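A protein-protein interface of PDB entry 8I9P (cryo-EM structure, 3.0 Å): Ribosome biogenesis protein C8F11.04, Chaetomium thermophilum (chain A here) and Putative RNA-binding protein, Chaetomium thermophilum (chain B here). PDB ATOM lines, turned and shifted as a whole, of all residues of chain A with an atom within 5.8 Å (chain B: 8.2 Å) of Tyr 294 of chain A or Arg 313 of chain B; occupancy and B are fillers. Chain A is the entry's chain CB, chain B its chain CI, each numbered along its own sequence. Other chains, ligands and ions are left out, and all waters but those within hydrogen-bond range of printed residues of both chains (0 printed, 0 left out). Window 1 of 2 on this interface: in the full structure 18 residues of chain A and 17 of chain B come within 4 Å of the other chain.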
ATOM      1  N   ARG A 279      13.362   4.544   5.070  1.00  0.00           N
ATOM      2  CA  ARG A 279      11.950   4.792   4.813  1.00  0.00           C
ATOM      3  C   ARG A 279      11.413   5.952   5.643  1.00  0.00           C
ATOM      4  O   ARG A 279      10.884   6.918   5.087  1.00  0.00           O
ATOM      5  CB  ARG A 279      11.139   3.515   5.078  1.00  0.00           C
ATOM      6  CG  ARG A 279       9.677   3.619   4.708  1.00  0.00           C
ATOM      7  CD  ARG A 279       9.213   2.344   4.043  1.00  0.00           C
ATOM      8  NE  ARG A 279       7.771   2.158   4.137  1.00  0.00           N
ATOM      9  CZ  ARG A 279       7.181   0.974   4.205  1.00  0.00           C
ATOM     10  NH1 ARG A 279       7.881  -0.149   4.200  1.00  0.00           N
ATOM     11  NH2 ARG A 279       5.854   0.913   4.260  1.00  0.00           N
ATOM     12  N   ASN A 280      11.528   5.880   6.968  1.00  0.00           N
ATOM     13  CA  ASN A 280      11.027   6.910   7.873  1.00  0.00           C
ATOM     14  C   ASN A 280      12.122   7.282   8.857  1.00  0.00           C
ATOM     15  O   ASN A 280      12.872   6.403   9.291  1.00  0.00           O
ATOM     16  CB  ASN A 280       9.815   6.420   8.678  1.00  0.00           C
ATOM     17  CG  ASN A 280       8.654   5.962   7.818  1.00  0.00           C
ATOM     18  OD1 ASN A 280       7.804   5.195   8.272  1.00  0.00           O
ATOM     19  ND2 ASN A 280       8.568   6.478   6.609  1.00  0.00           N
ATOM     20  N   PHE A 281      12.204   8.560   9.235  1.00  0.00           N
ATOM     21  CA  PHE A 281      12.858   8.939  10.492  1.00  0.00           C
ATOM     22  C   PHE A 281      11.811   9.605  11.378  1.00  0.00           C
ATOM     23  O   PHE A 281      11.478  10.777  11.211  1.00  0.00           O
ATOM     24  CB  PHE A 281      14.114   9.837  10.354  1.00  0.00           C
ATOM     25  CG  PHE A 281      15.337   9.131   9.817  1.00  0.00           C
ATOM     26  CD1 PHE A 281      15.282   8.282   8.731  1.00  0.00           C
ATOM     27  CD2 PHE A 281      16.533   9.233  10.502  1.00  0.00           C
ATOM     28  CE1 PHE A 281      16.408   7.629   8.294  1.00  0.00           C
ATOM     29  CE2 PHE A 281      17.666   8.579  10.063  1.00  0.00           C
ATOM     30  CZ  PHE A 281      17.600   7.775   8.956  1.00  0.00           C
ATOM     31  N   TYR A 282      11.297   8.843  12.331  1.00  0.00           N
ATOM     32  CA  TYR A 282      10.320   9.362  13.271  1.00  0.00           C
ATOM     33  C   TYR A 282      11.008   9.917  14.507  1.00  0.00           C
ATOM     34  O   TYR A 282      11.726   9.205  15.215  1.00  0.00           O
ATOM     35  CB  TYR A 282       9.341   8.260  13.678  1.00  0.00           C
ATOM     36  CG  TYR A 282       8.412   7.828  12.573  1.00  0.00           C
ATOM     37  CD1 TYR A 282       8.268   8.590  11.427  1.00  0.00           C
ATOM     38  CD2 TYR A 282       7.718   6.633  12.653  1.00  0.00           C
ATOM     39  CE1 TYR A 282       7.424   8.209  10.418  1.00  0.00           C
ATOM     40  CE2 TYR A 282       6.884   6.233  11.633  1.00  0.00           C
ATOM     41  CZ  TYR A 282       6.744   7.023  10.519  1.00  0.00           C
ATOM     42  OH  TYR A 282       5.908   6.632   9.499  1.00  0.00           O
ATOM     43  N   PRO A 292       6.811  12.536  11.804  1.00  0.00           N
ATOM     44  CA  PRO A 292       7.620  11.962  10.723  1.00  0.00           C
ATOM     45  C   PRO A 292       8.644  12.908  10.127  1.00  0.00           C
ATOM     46  O   PRO A 292       8.473  14.128  10.159  1.00  0.00           O
ATOM     47  CB  PRO A 292       6.571  11.572   9.673  1.00  0.00           C
ATOM     48  CG  PRO A 292       5.383  12.433   9.949  1.00  0.00           C
ATOM     49  CD  PRO A 292       5.506  13.023  11.330  1.00  0.00           C
ATOM     50  N   ILE A 293       9.728  12.334   9.615  1.00  0.00           N
ATOM     51  CA  ILE A 293      10.545  12.917   8.556  1.00  0.00           C
ATOM     52  C   ILE A 293      10.562  11.846   7.470  1.00  0.00           C
ATOM     53  O   ILE A 293      11.271  10.837   7.571  1.00  0.00           O
ATOM     54  CB  ILE A 293      11.960  13.285   9.016  1.00  0.00           C
ATOM     55  CG1 ILE A 293      11.962  13.879  10.431  1.00  0.00           C
ATOM     56  CG2 ILE A 293      12.612  14.256   8.034  1.00  0.00           C
ATOM     57  CD1 ILE A 293      11.435  15.295  10.528  1.00  0.00           C
ATOM     58  N   TYR A 294       9.734  12.032   6.446  1.00  0.00           N
ATOM     59  CA  TYR A 294       9.463  10.968   5.497  1.00  0.00           C
ATOM     60  C   TYR A 294      10.380  11.117   4.285  1.00  0.00           C
ATOM     61  O   TYR A 294      10.526  12.200   3.713  1.00  0.00           O
ATOM     62  CB  TYR A 294       7.995  11.006   5.074  1.00  0.00           C
ATOM     63  CG  TYR A 294       7.314   9.661   4.999  1.00  0.00           C
ATOM     64  CD1 TYR A 294       7.668   8.724   4.043  1.00  0.00           C
ATOM     65  CD2 TYR A 294       6.322   9.324   5.913  1.00  0.00           C
ATOM     66  CE1 TYR A 294       7.042   7.492   3.993  1.00  0.00           C
ATOM     67  CE2 TYR A 294       5.688   8.099   5.864  1.00  0.00           C
ATOM     68  CZ  TYR A 294       6.051   7.187   4.899  1.00  0.00           C
ATOM     69  OH  TYR A 294       5.430   5.961   4.845  1.00  0.00           O
ATOM     70  N   GLN A 295      10.999  10.007   3.882  1.00  0.00           N
ATOM     71  CA  GLN A 295      12.086  10.075   2.912  1.00  0.00           C
ATOM     72  C   GLN A 295      11.833   9.199   1.688  1.00  0.00           C
ATOM     73  O   GLN A 295      12.788   8.751   1.043  1.00  0.00           O
ATOM     74  CB  GLN A 295      13.412   9.657   3.552  1.00  0.00           C
ATOM     75  CG  GLN A 295      13.963  10.583   4.634  1.00  0.00           C
ATOM     76  CD  GLN A 295      13.687  12.049   4.378  1.00  0.00           C
ATOM     77  OE1 GLN A 295      12.977  12.701   5.143  1.00  0.00           O
ATOM     78  NE2 GLN A 295      14.274  12.585   3.313  1.00  0.00           N
ATOM     79  N   THR A 296      10.574   8.938   1.342  1.00  0.00           N
ATOM     80  CA  THR A 296      10.282   7.979   0.283  1.00  0.00           C
ATOM     81  C   THR A 296       9.598   8.637  -0.906  1.00  0.00           C
ATOM     82  O   THR A 296       8.648   9.410  -0.744  1.00  0.00           O
ATOM     83  CB  THR A 296       9.382   6.852   0.780  1.00  0.00           C
ATOM     84  OG1 THR A 296       8.104   7.394   1.129  1.00  0.00           O
ATOM     85  CG2 THR A 296       9.987   6.179   1.988  1.00  0.00           C
ATOM     86  N   VAL B 306       1.195   0.460  -1.814  1.00  0.00           N
ATOM     87  CA  VAL B 306       1.046   1.912  -1.797  1.00  0.00           C
ATOM     88  C   VAL B 306      -0.352   2.310  -1.334  1.00  0.00           C
ATOM     89  O   VAL B 306      -0.524   3.380  -0.742  1.00  0.00           O
ATOM     90  CB  VAL B 306       1.398   2.532  -3.163  1.00  0.00           C
ATOM     91  CG1 VAL B 306       2.913   2.517  -3.382  1.00  0.00           C
ATOM     92  CG2 VAL B 306       0.668   1.843  -4.289  1.00  0.00           C
ATOM     93  N   ALA B 307      -1.364   1.460  -1.547  1.00  0.00           N
ATOM     94  CA  ALA B 307      -2.697   1.768  -1.026  1.00  0.00           C
ATOM     95  C   ALA B 307      -2.718   1.738   0.501  1.00  0.00           C
ATOM     96  O   ALA B 307      -3.279   2.641   1.150  1.00  0.00           O
ATOM     97  CB  ALA B 307      -3.725   0.798  -1.605  1.00  0.00           C
ATOM     98  N   LYS B 308      -2.105   0.700   1.092  1.00  0.00           N
ATOM     99  CA  LYS B 308      -1.985   0.628   2.545  1.00  0.00           C
ATOM    100  C   LYS B 308      -1.187   1.809   3.081  1.00  0.00           C
ATOM    101  O   LYS B 308      -1.574   2.434   4.083  1.00  0.00           O
ATOM    102  CB  LYS B 308      -1.338  -0.693   2.960  1.00  0.00           C
ATOM    103  CG  LYS B 308      -2.253  -1.613   3.752  1.00  0.00           C
ATOM    104  CD  LYS B 308      -3.362  -2.183   2.885  1.00  0.00           C
ATOM    105  CE  LYS B 308      -4.287  -3.076   3.695  1.00  0.00           C
ATOM    106  NZ  LYS B 308      -3.786  -4.477   3.749  1.00  0.00           N
ATOM    107  N   GLU B 309      -0.098   2.154   2.386  1.00  0.00           N
ATOM    108  CA  GLU B 309       0.708   3.307   2.763  1.00  0.00           C
ATOM    109  C   GLU B 309      -0.121   4.585   2.758  1.00  0.00           C
ATOM    110  O   GLU B 309      -0.058   5.371   3.710  1.00  0.00           O
ATOM    111  CB  GLU B 309       1.917   3.420   1.826  1.00  0.00           C
ATOM    112  CG  GLU B 309       2.609   4.779   1.799  1.00  0.00           C
ATOM    113  CD  GLU B 309       2.140   5.661   0.652  1.00  0.00           C
ATOM    114  OE1 GLU B 309       1.719   5.115  -0.388  1.00  0.00           O
ATOM    115  OE2 GLU B 309       2.212   6.900   0.783  1.00  0.00           O
ATOM    116  N   GLU B 310      -0.959   4.782   1.732  1.00  0.00           N
ATOM    117  CA  GLU B 310      -1.631   6.072   1.638  1.00  0.00           C
ATOM    118  C   GLU B 310      -2.750   6.222   2.666  1.00  0.00           C
ATOM    119  O   GLU B 310      -2.873   7.308   3.245  1.00  0.00           O
ATOM    120  CB  GLU B 310      -2.155   6.365   0.222  1.00  0.00           C
ATOM    121  CG  GLU B 310      -3.036   5.342  -0.449  1.00  0.00           C
ATOM    122  CD  GLU B 310      -4.502   5.497  -0.098  1.00  0.00           C
ATOM    123  OE1 GLU B 310      -4.883   6.573   0.408  1.00  0.00           O
ATOM    124  OE2 GLU B 310      -5.273   4.543  -0.329  1.00  0.00           O
ATOM    125  N   GLN B 311      -3.568   5.190   2.957  1.00  0.00           N
ATOM    126  CA  GLN B 311      -4.627   5.572   3.901  1.00  0.00           C
ATOM    127  C   GLN B 311      -4.125   5.456   5.341  1.00  0.00           C
ATOM    128  O   GLN B 311      -4.683   6.101   6.241  1.00  0.00           O
ATOM    129  CB  GLN B 311      -5.965   4.810   3.753  1.00  0.00           C
ATOM    130  CG  GLN B 311      -6.289   3.412   4.373  1.00  0.00           C
ATOM    131  CD  GLN B 311      -5.279   2.321   4.269  1.00  0.00           C
ATOM    132  OE1 GLN B 311      -4.251   2.480   3.671  1.00  0.00           O
ATOM    133  NE2 GLN B 311      -5.587   1.177   4.871  1.00  0.00           N
ATOM    134  N   ARG B 312      -3.032   4.708   5.590  1.00  0.00           N
ATOM    135  CA  ARG B 312      -2.457   4.814   6.931  1.00  0.00           C
ATOM    136  C   ARG B 312      -1.743   6.152   7.116  1.00  0.00           C
ATOM    137  O   ARG B 312      -1.763   6.713   8.221  1.00  0.00           O
ATOM    138  CB  ARG B 312      -1.529   3.631   7.236  1.00  0.00           C
ATOM    139  CG  ARG B 312      -0.136   3.666   6.635  1.00  0.00           C
ATOM    140  CD  ARG B 312       0.548   2.324   6.838  1.00  0.00           C
ATOM    141  NE  ARG B 312       1.991   2.398   6.652  1.00  0.00           N
ATOM    142  CZ  ARG B 312       2.827   1.406   6.918  1.00  0.00           C
ATOM    143  NH1 ARG B 312       2.398   0.247   7.392  1.00  0.00           N
ATOM    144  NH2 ARG B 312       4.127   1.576   6.696  1.00  0.00           N
ATOM    145  N   ARG B 313      -1.164   6.706   6.041  1.00  0.00           N
ATOM    146  CA  ARG B 313      -0.659   8.073   6.094  1.00  0.00           C
ATOM    147  C   ARG B 313      -1.788   9.068   6.302  1.00  0.00           C
ATOM    148  O   ARG B 313      -1.604  10.084   6.973  1.00  0.00           O
ATOM    149  CB  ARG B 313       0.105   8.411   4.814  1.00  0.00           C
ATOM    150  CG  ARG B 313       1.546   7.937   4.770  1.00  0.00           C
ATOM    151  CD  ARG B 313       2.357   8.844   3.868  1.00  0.00           C
ATOM    152  NE  ARG B 313       3.171   8.087   2.924  1.00  0.00           N
ATOM    153  CZ  ARG B 313       4.291   8.535   2.377  1.00  0.00           C
ATOM    154  NH1 ARG B 313       4.776   9.730   2.672  1.00  0.00           N
ATOM    155  NH2 ARG B 313       4.941   7.765   1.509  1.00  0.00           N
ATOM    156  N   ALA B 314      -2.962   8.798   5.725  1.00  0.00           N
ATOM    157  CA  ALA B 314      -4.111   9.679   5.923  1.00  0.00           C
ATOM    158  C   ALA B 314      -4.581   9.672   7.375  1.00  0.00           C
ATOM    159  O   ALA B 314      -4.881  10.730   7.945  1.00  0.00           O
ATOM    160  CB  ALA B 314      -5.248   9.271   4.988  1.00  0.00           C
ATOM    161  N   ALA B 315      -4.653   8.485   7.988  1.00  0.00           N
ATOM    162  CA  ALA B 315      -5.041   8.400   9.396  1.00  0.00           C
ATOM    163  C   ALA B 315      -4.012   9.076  10.299  1.00  0.00           C
ATOM    164  O   ALA B 315      -4.372   9.815  11.230  1.00  0.00           O
ATOM    165  CB  ALA B 315      -5.234   6.939   9.800  1.00  0.00           C
ATOM    166  N   ARG B 316      -2.721   8.849  10.027  1.00  0.00           N
ATOM    167  CA  ARG B 316      -1.669   9.523  10.780  1.00  0.00           C
ATOM    168  C   ARG B 316      -1.718  11.033  10.571  1.00  0.00           C
ATOM    169  O   ARG B 316      -1.459  11.805  11.500  1.00  0.00           O
ATOM    170  CB  ARG B 316      -0.308   8.962  10.371  1.00  0.00           C
ATOM    171  CG  ARG B 316       0.872   9.548  11.117  1.00  0.00           C
ATOM    172  CD  ARG B 316       1.701   8.451  11.751  1.00  0.00           C
ATOM    173  NE  ARG B 316       1.779   7.280  10.886  1.00  0.00           N
ATOM    174  CZ  ARG B 316       2.794   7.017  10.077  1.00  0.00           C
ATOM    175  NH1 ARG B 316       3.807   7.856   9.947  1.00  0.00           N
ATOM    176  NH2 ARG B 316       2.784   5.892   9.368  1.00  0.00           N
ATOM    177  N   ALA B 317      -2.059  11.469   9.357  1.00  0.00           N
ATOM    178  CA  ALA B 317      -2.194  12.890   9.075  1.00  0.00           C
ATOM    179  C   ALA B 317      -3.343  13.500   9.860  1.00  0.00           C
ATOM    180  O   ALA B 317      -3.235  14.624  10.346  1.00  0.00           O
ATOM    181  CB  ALA B 317      -2.393  13.109   7.576  1.00  0.00           C
ATOM    182  N   GLU B 318      -4.453  12.776  10.000  1.00  0.00           N
ATOM    183  CA  GLU B 318      -5.539  13.284  10.837  1.00  0.00           C
ATOM    184  C   GLU B 318      -5.077  13.392  12.288  1.00  0.00           C
ATOM    185  O   GLU B 318      -5.356  14.389  12.972  1.00  0.00           O
ATOM    186  CB  GLU B 318      -6.792  12.402  10.633  1.00  0.00           C
ATOM    187  CG  GLU B 318      -8.068  12.535  11.537  1.00  0.00           C
ATOM    188  CD  GLU B 318      -7.958  12.156  13.016  1.00  0.00           C
ATOM    189  OE1 GLU B 318      -6.973  11.526  13.441  1.00  0.00           O
ATOM    190  OE2 GLU B 318      -8.956  12.360  13.736  1.00  0.00           O
ATOM    191  N   LYS B 319      -4.315  12.392  12.753  1.00  0.00           N
ATOM    192  CA  LYS B 319      -3.852  12.385  14.141  1.00  0.00           C
ATOM    193  C   LYS B 319      -2.891  13.537  14.435  1.00  0.00           C
ATOM    194  O   LYS B 319      -2.959  14.146  15.509  1.00  0.00           O
ATOM    195  CB  LYS B 319      -3.196  11.044  14.470  1.00  0.00           C
ATOM    196  CG  LYS B 319      -2.751  10.912  15.920  1.00  0.00           C
ATOM    197  CD  LYS B 319      -2.079   9.576  16.181  1.00  0.00           C
ATOM    198  CE  LYS B 319      -1.858   9.338  17.669  1.00  0.00           C
ATOM    199  NZ  LYS B 319      -2.348  10.465  18.515  1.00  0.00           N
ATOM    200  N   LEU B 320      -1.993  13.859  13.503  1.00  0.00           N
ATOM    201  CA  LEU B 320      -1.041  14.948  13.720  1.00  0.00           C
ATOM    202  C   LEU B 320      -1.515  16.297  13.178  1.00  0.00           C
ATOM    203  O   LEU B 320      -0.824  17.298  13.377  1.00  0.00           O
ATOM    204  CB  LEU B 320       0.335  14.608  13.134  1.00  0.00           C
ATOM    205  CG  LEU B 320       0.872  13.179  13.185  1.00  0.00           C
ATOM    206  CD1 LEU B 320       1.929  12.981  12.119  1.00  0.00           C
ATOM    207  CD2 LEU B 320       1.447  12.883  14.561  1.00  0.00           C
ATOM    208  N   LYS B 321      -2.657  16.346  12.489  1.00  0.00           N
ATOM    209  CA  LYS B 321      -3.393  17.591  12.321  1.00  0.00           C
ATOM    210  C   LYS B 321      -4.301  17.892  13.499  1.00  0.00           C
ATOM    211  O   LYS B 321      -4.795  19.021  13.608  1.00  0.00           O
ATOM    212  CB  LYS B 321      -4.247  17.565  11.041  1.00  0.00           C
ATOM    213  CG  LYS B 321      -3.750  18.338   9.783  1.00  0.00           C
ATOM    214  CD  LYS B 321      -2.257  18.365   9.393  1.00  0.00           C
ATOM    215  CE  LYS B 321      -1.623  17.000   9.213  1.00  0.00           C
ATOM    216  NZ  LYS B 321      -0.183  17.052   8.853  1.00  0.00           N
ATOM    217  N   TYR B 325       0.957  19.531  12.508  1.00  0.00           N
ATOM    218  CA  TYR B 325       2.257  19.314  11.889  1.00  0.00           C
ATOM    219  C   TYR B 325       2.034  18.922  10.438  1.00  0.00           C
ATOM    220  O   TYR B 325       1.493  17.848  10.167  1.00  0.00           O
ATOM    221  CB  TYR B 325       3.053  18.222  12.618  1.00  0.00           C
ATOM    222  CG  TYR B 325       4.443  18.011  12.063  1.00  0.00           C
ATOM    223  CD1 TYR B 325       5.335  19.069  11.956  1.00  0.00           C
ATOM    224  CD2 TYR B 325       4.863  16.754  11.646  1.00  0.00           C
ATOM    225  CE1 TYR B 325       6.609  18.883  11.448  1.00  0.00           C
ATOM    226  CE2 TYR B 325       6.135  16.557  11.137  1.00  0.00           C
ATOM    227  CZ  TYR B 325       7.003  17.624  11.038  1.00  0.00           C
ATOM    228  OH  TYR B 325       8.268  17.426  10.530  1.00  0.00           O
ATOM    229  N   PHE B 327       2.819  17.944   6.473  1.00  0.00           N
ATOM    230  CA  PHE B 327       3.701  17.151   5.624  1.00  0.00           C
ATOM    231  C   PHE B 327       3.185  17.091   4.189  1.00  0.00           C
ATOM    232  O   PHE B 327       2.034  17.426   3.895  1.00  0.00           O
ATOM    233  CB  PHE B 327       3.899  15.739   6.178  1.00  0.00           C
ATOM    234  CG  PHE B 327       5.314  15.451   6.548  1.00  0.00           C
ATOM    235  CD1 PHE B 327       5.919  16.109   7.600  1.00  0.00           C
ATOM    236  CD2 PHE B 327       6.062  14.558   5.801  1.00  0.00           C
ATOM    237  CE1 PHE B 327       7.231  15.858   7.918  1.00  0.00           C
ATOM    238  CE2 PHE B 327       7.376  14.307   6.118  1.00  0.00           C
ATOM    239  CZ  PHE B 327       7.960  14.957   7.177  1.00  0.00           C
ATOM    240  N   GLU B 328       4.069  16.647   3.296  1.00  0.00           N
ATOM    241  CA  GLU B 328       3.837  16.635   1.856  1.00  0.00           C
ATOM    242  C   GLU B 328       4.324  15.296   1.307  1.00  0.00           C
ATOM    243  O   GLU B 328       4.552  14.344   2.062  1.00  0.00           O
ATOM    244  CB  GLU B 328       4.557  17.801   1.156  1.00  0.00           C
ATOM    245  CG  GLU B 328       4.383  19.176   1.787  1.00  0.00           C
ATOM    246  CD  GLU B 328       5.446  19.475   2.831  1.00  0.00           C
ATOM    247  OE1 GLU B 328       6.368  18.648   2.996  1.00  0.00           O
ATOM    248  OE2 GLU B 328       5.357  20.534   3.488  1.00  0.00           O
ATOM    249  N   ALA B 329       4.454  15.234  -0.020  1.00  0.00           N
ATOM    250  CA  ALA B 329       5.014  14.096  -0.765  1.00  0.00           C
ATOM    251  C   ALA B 329       4.260  12.783  -0.547  1.00  0.00           C
ATOM    252  O   ALA B 329       4.736  11.719  -0.941  1.00  0.00           O
ATOM    253  CB  ALA B 329       6.498  13.912  -0.426  1.00  0.00           C
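The side-chain hydroxyl (OH) of Tyr 282 of chain A sits at hydrogen-bond distance from the guanidinium group (NH1) of Arg 316 of chain B.
O of Pro 292 of chain A lies within hydrogen-bond range of OH of Tyr 325 of chain B (3.3 Å).
The side-chain hydroxyl of Thr 296 of chain A sits at hydrogen-bond distance from the guanidinium group of Arg 313 of chain B, at 3.2 Å.
NH2 of Arg 312 of chain B lies close to NH2 of Arg 279 of chain A, 3.1 Å away.
Of the printed residues of chain B, Tyr 282 of chain A touches Arg 316 (2.5 Å).
Tyr 294 of chain A touches two residues of chain B.
Gln 311 of chain B touches none of the printed residues of chain A.
Of chain A, only Tyr 294 (3.3 Å) and Thr 296 (3.2 Å) come within 4 Å of Arg 313 of chain B.
Of the printed residues of chain A, Arg 316 of chain B touches Tyr 282.
Printed residues of chain A within 4 Å of Leu 320 of chain B: Pro 292.
Of the printed residues of chain A, Phe 327 of chain B touches Pro 292, Ile 293 and Tyr 294.
Glu 328 of chain B touches none of the printed residues of chain A.
Of the 20 printed residues of chain B, 6 touch a printed residue of chain A.
Hydrophobic or aromatic side chains of chain B within 4 Å of the printed part of chain A: Leu 320, Tyr 325 and Phe 327.
Of the 9 printed residues of chain A, 6 touch a printed residue of chain B.
Hydrophobic or aromatic side chains of chain A that line the printed part of chain B: Tyr 282, Pro 292, Ile 293 and Tyr 294.
Among the printed residues, pairs that only touch across the chains: Pro 292 of chain A with Leu 320 of chain B (3.7 Å), Pro 292 of chain A with Phe 327 of chain B (3.1 Å), Ile 293 of chain A with Tyr 325 of chain B (3.8 Å), Ile 293 of chain A with Phe 327 of chain B (3.6 Å), Tyr 294 of chain A with Arg 313 of chain B (3.3 Å) and Tyr 294 of chain A with Phe 327 of chain B (3.3 Å).
The backbone NH (N) of Gln 295 of chain A sits at hydrogen-bond distance from the backbone carbonyl oxygen (O) of Arg 279 of chain A.
The side-chain amide oxygen of Asn 280 of chain A is in hydrogen-bond range of the side-chain hydroxyl of Tyr 282 of chain A.
N of Ile 293 of chain A lies within hydrogen-bond range of O of Phe 281 of chain A, at 2.8 Å.
The guanidinium group (NE) of Arg 313 of chain B lies within salt-bridge range of the side-chain carboxylate (OE2) of Glu 309 of chain B, at 2.6 Å.
O of Leu 320 of chain B lies within hydrogen-bond range of N of Tyr 325 of chain B, at 3.0 Å.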
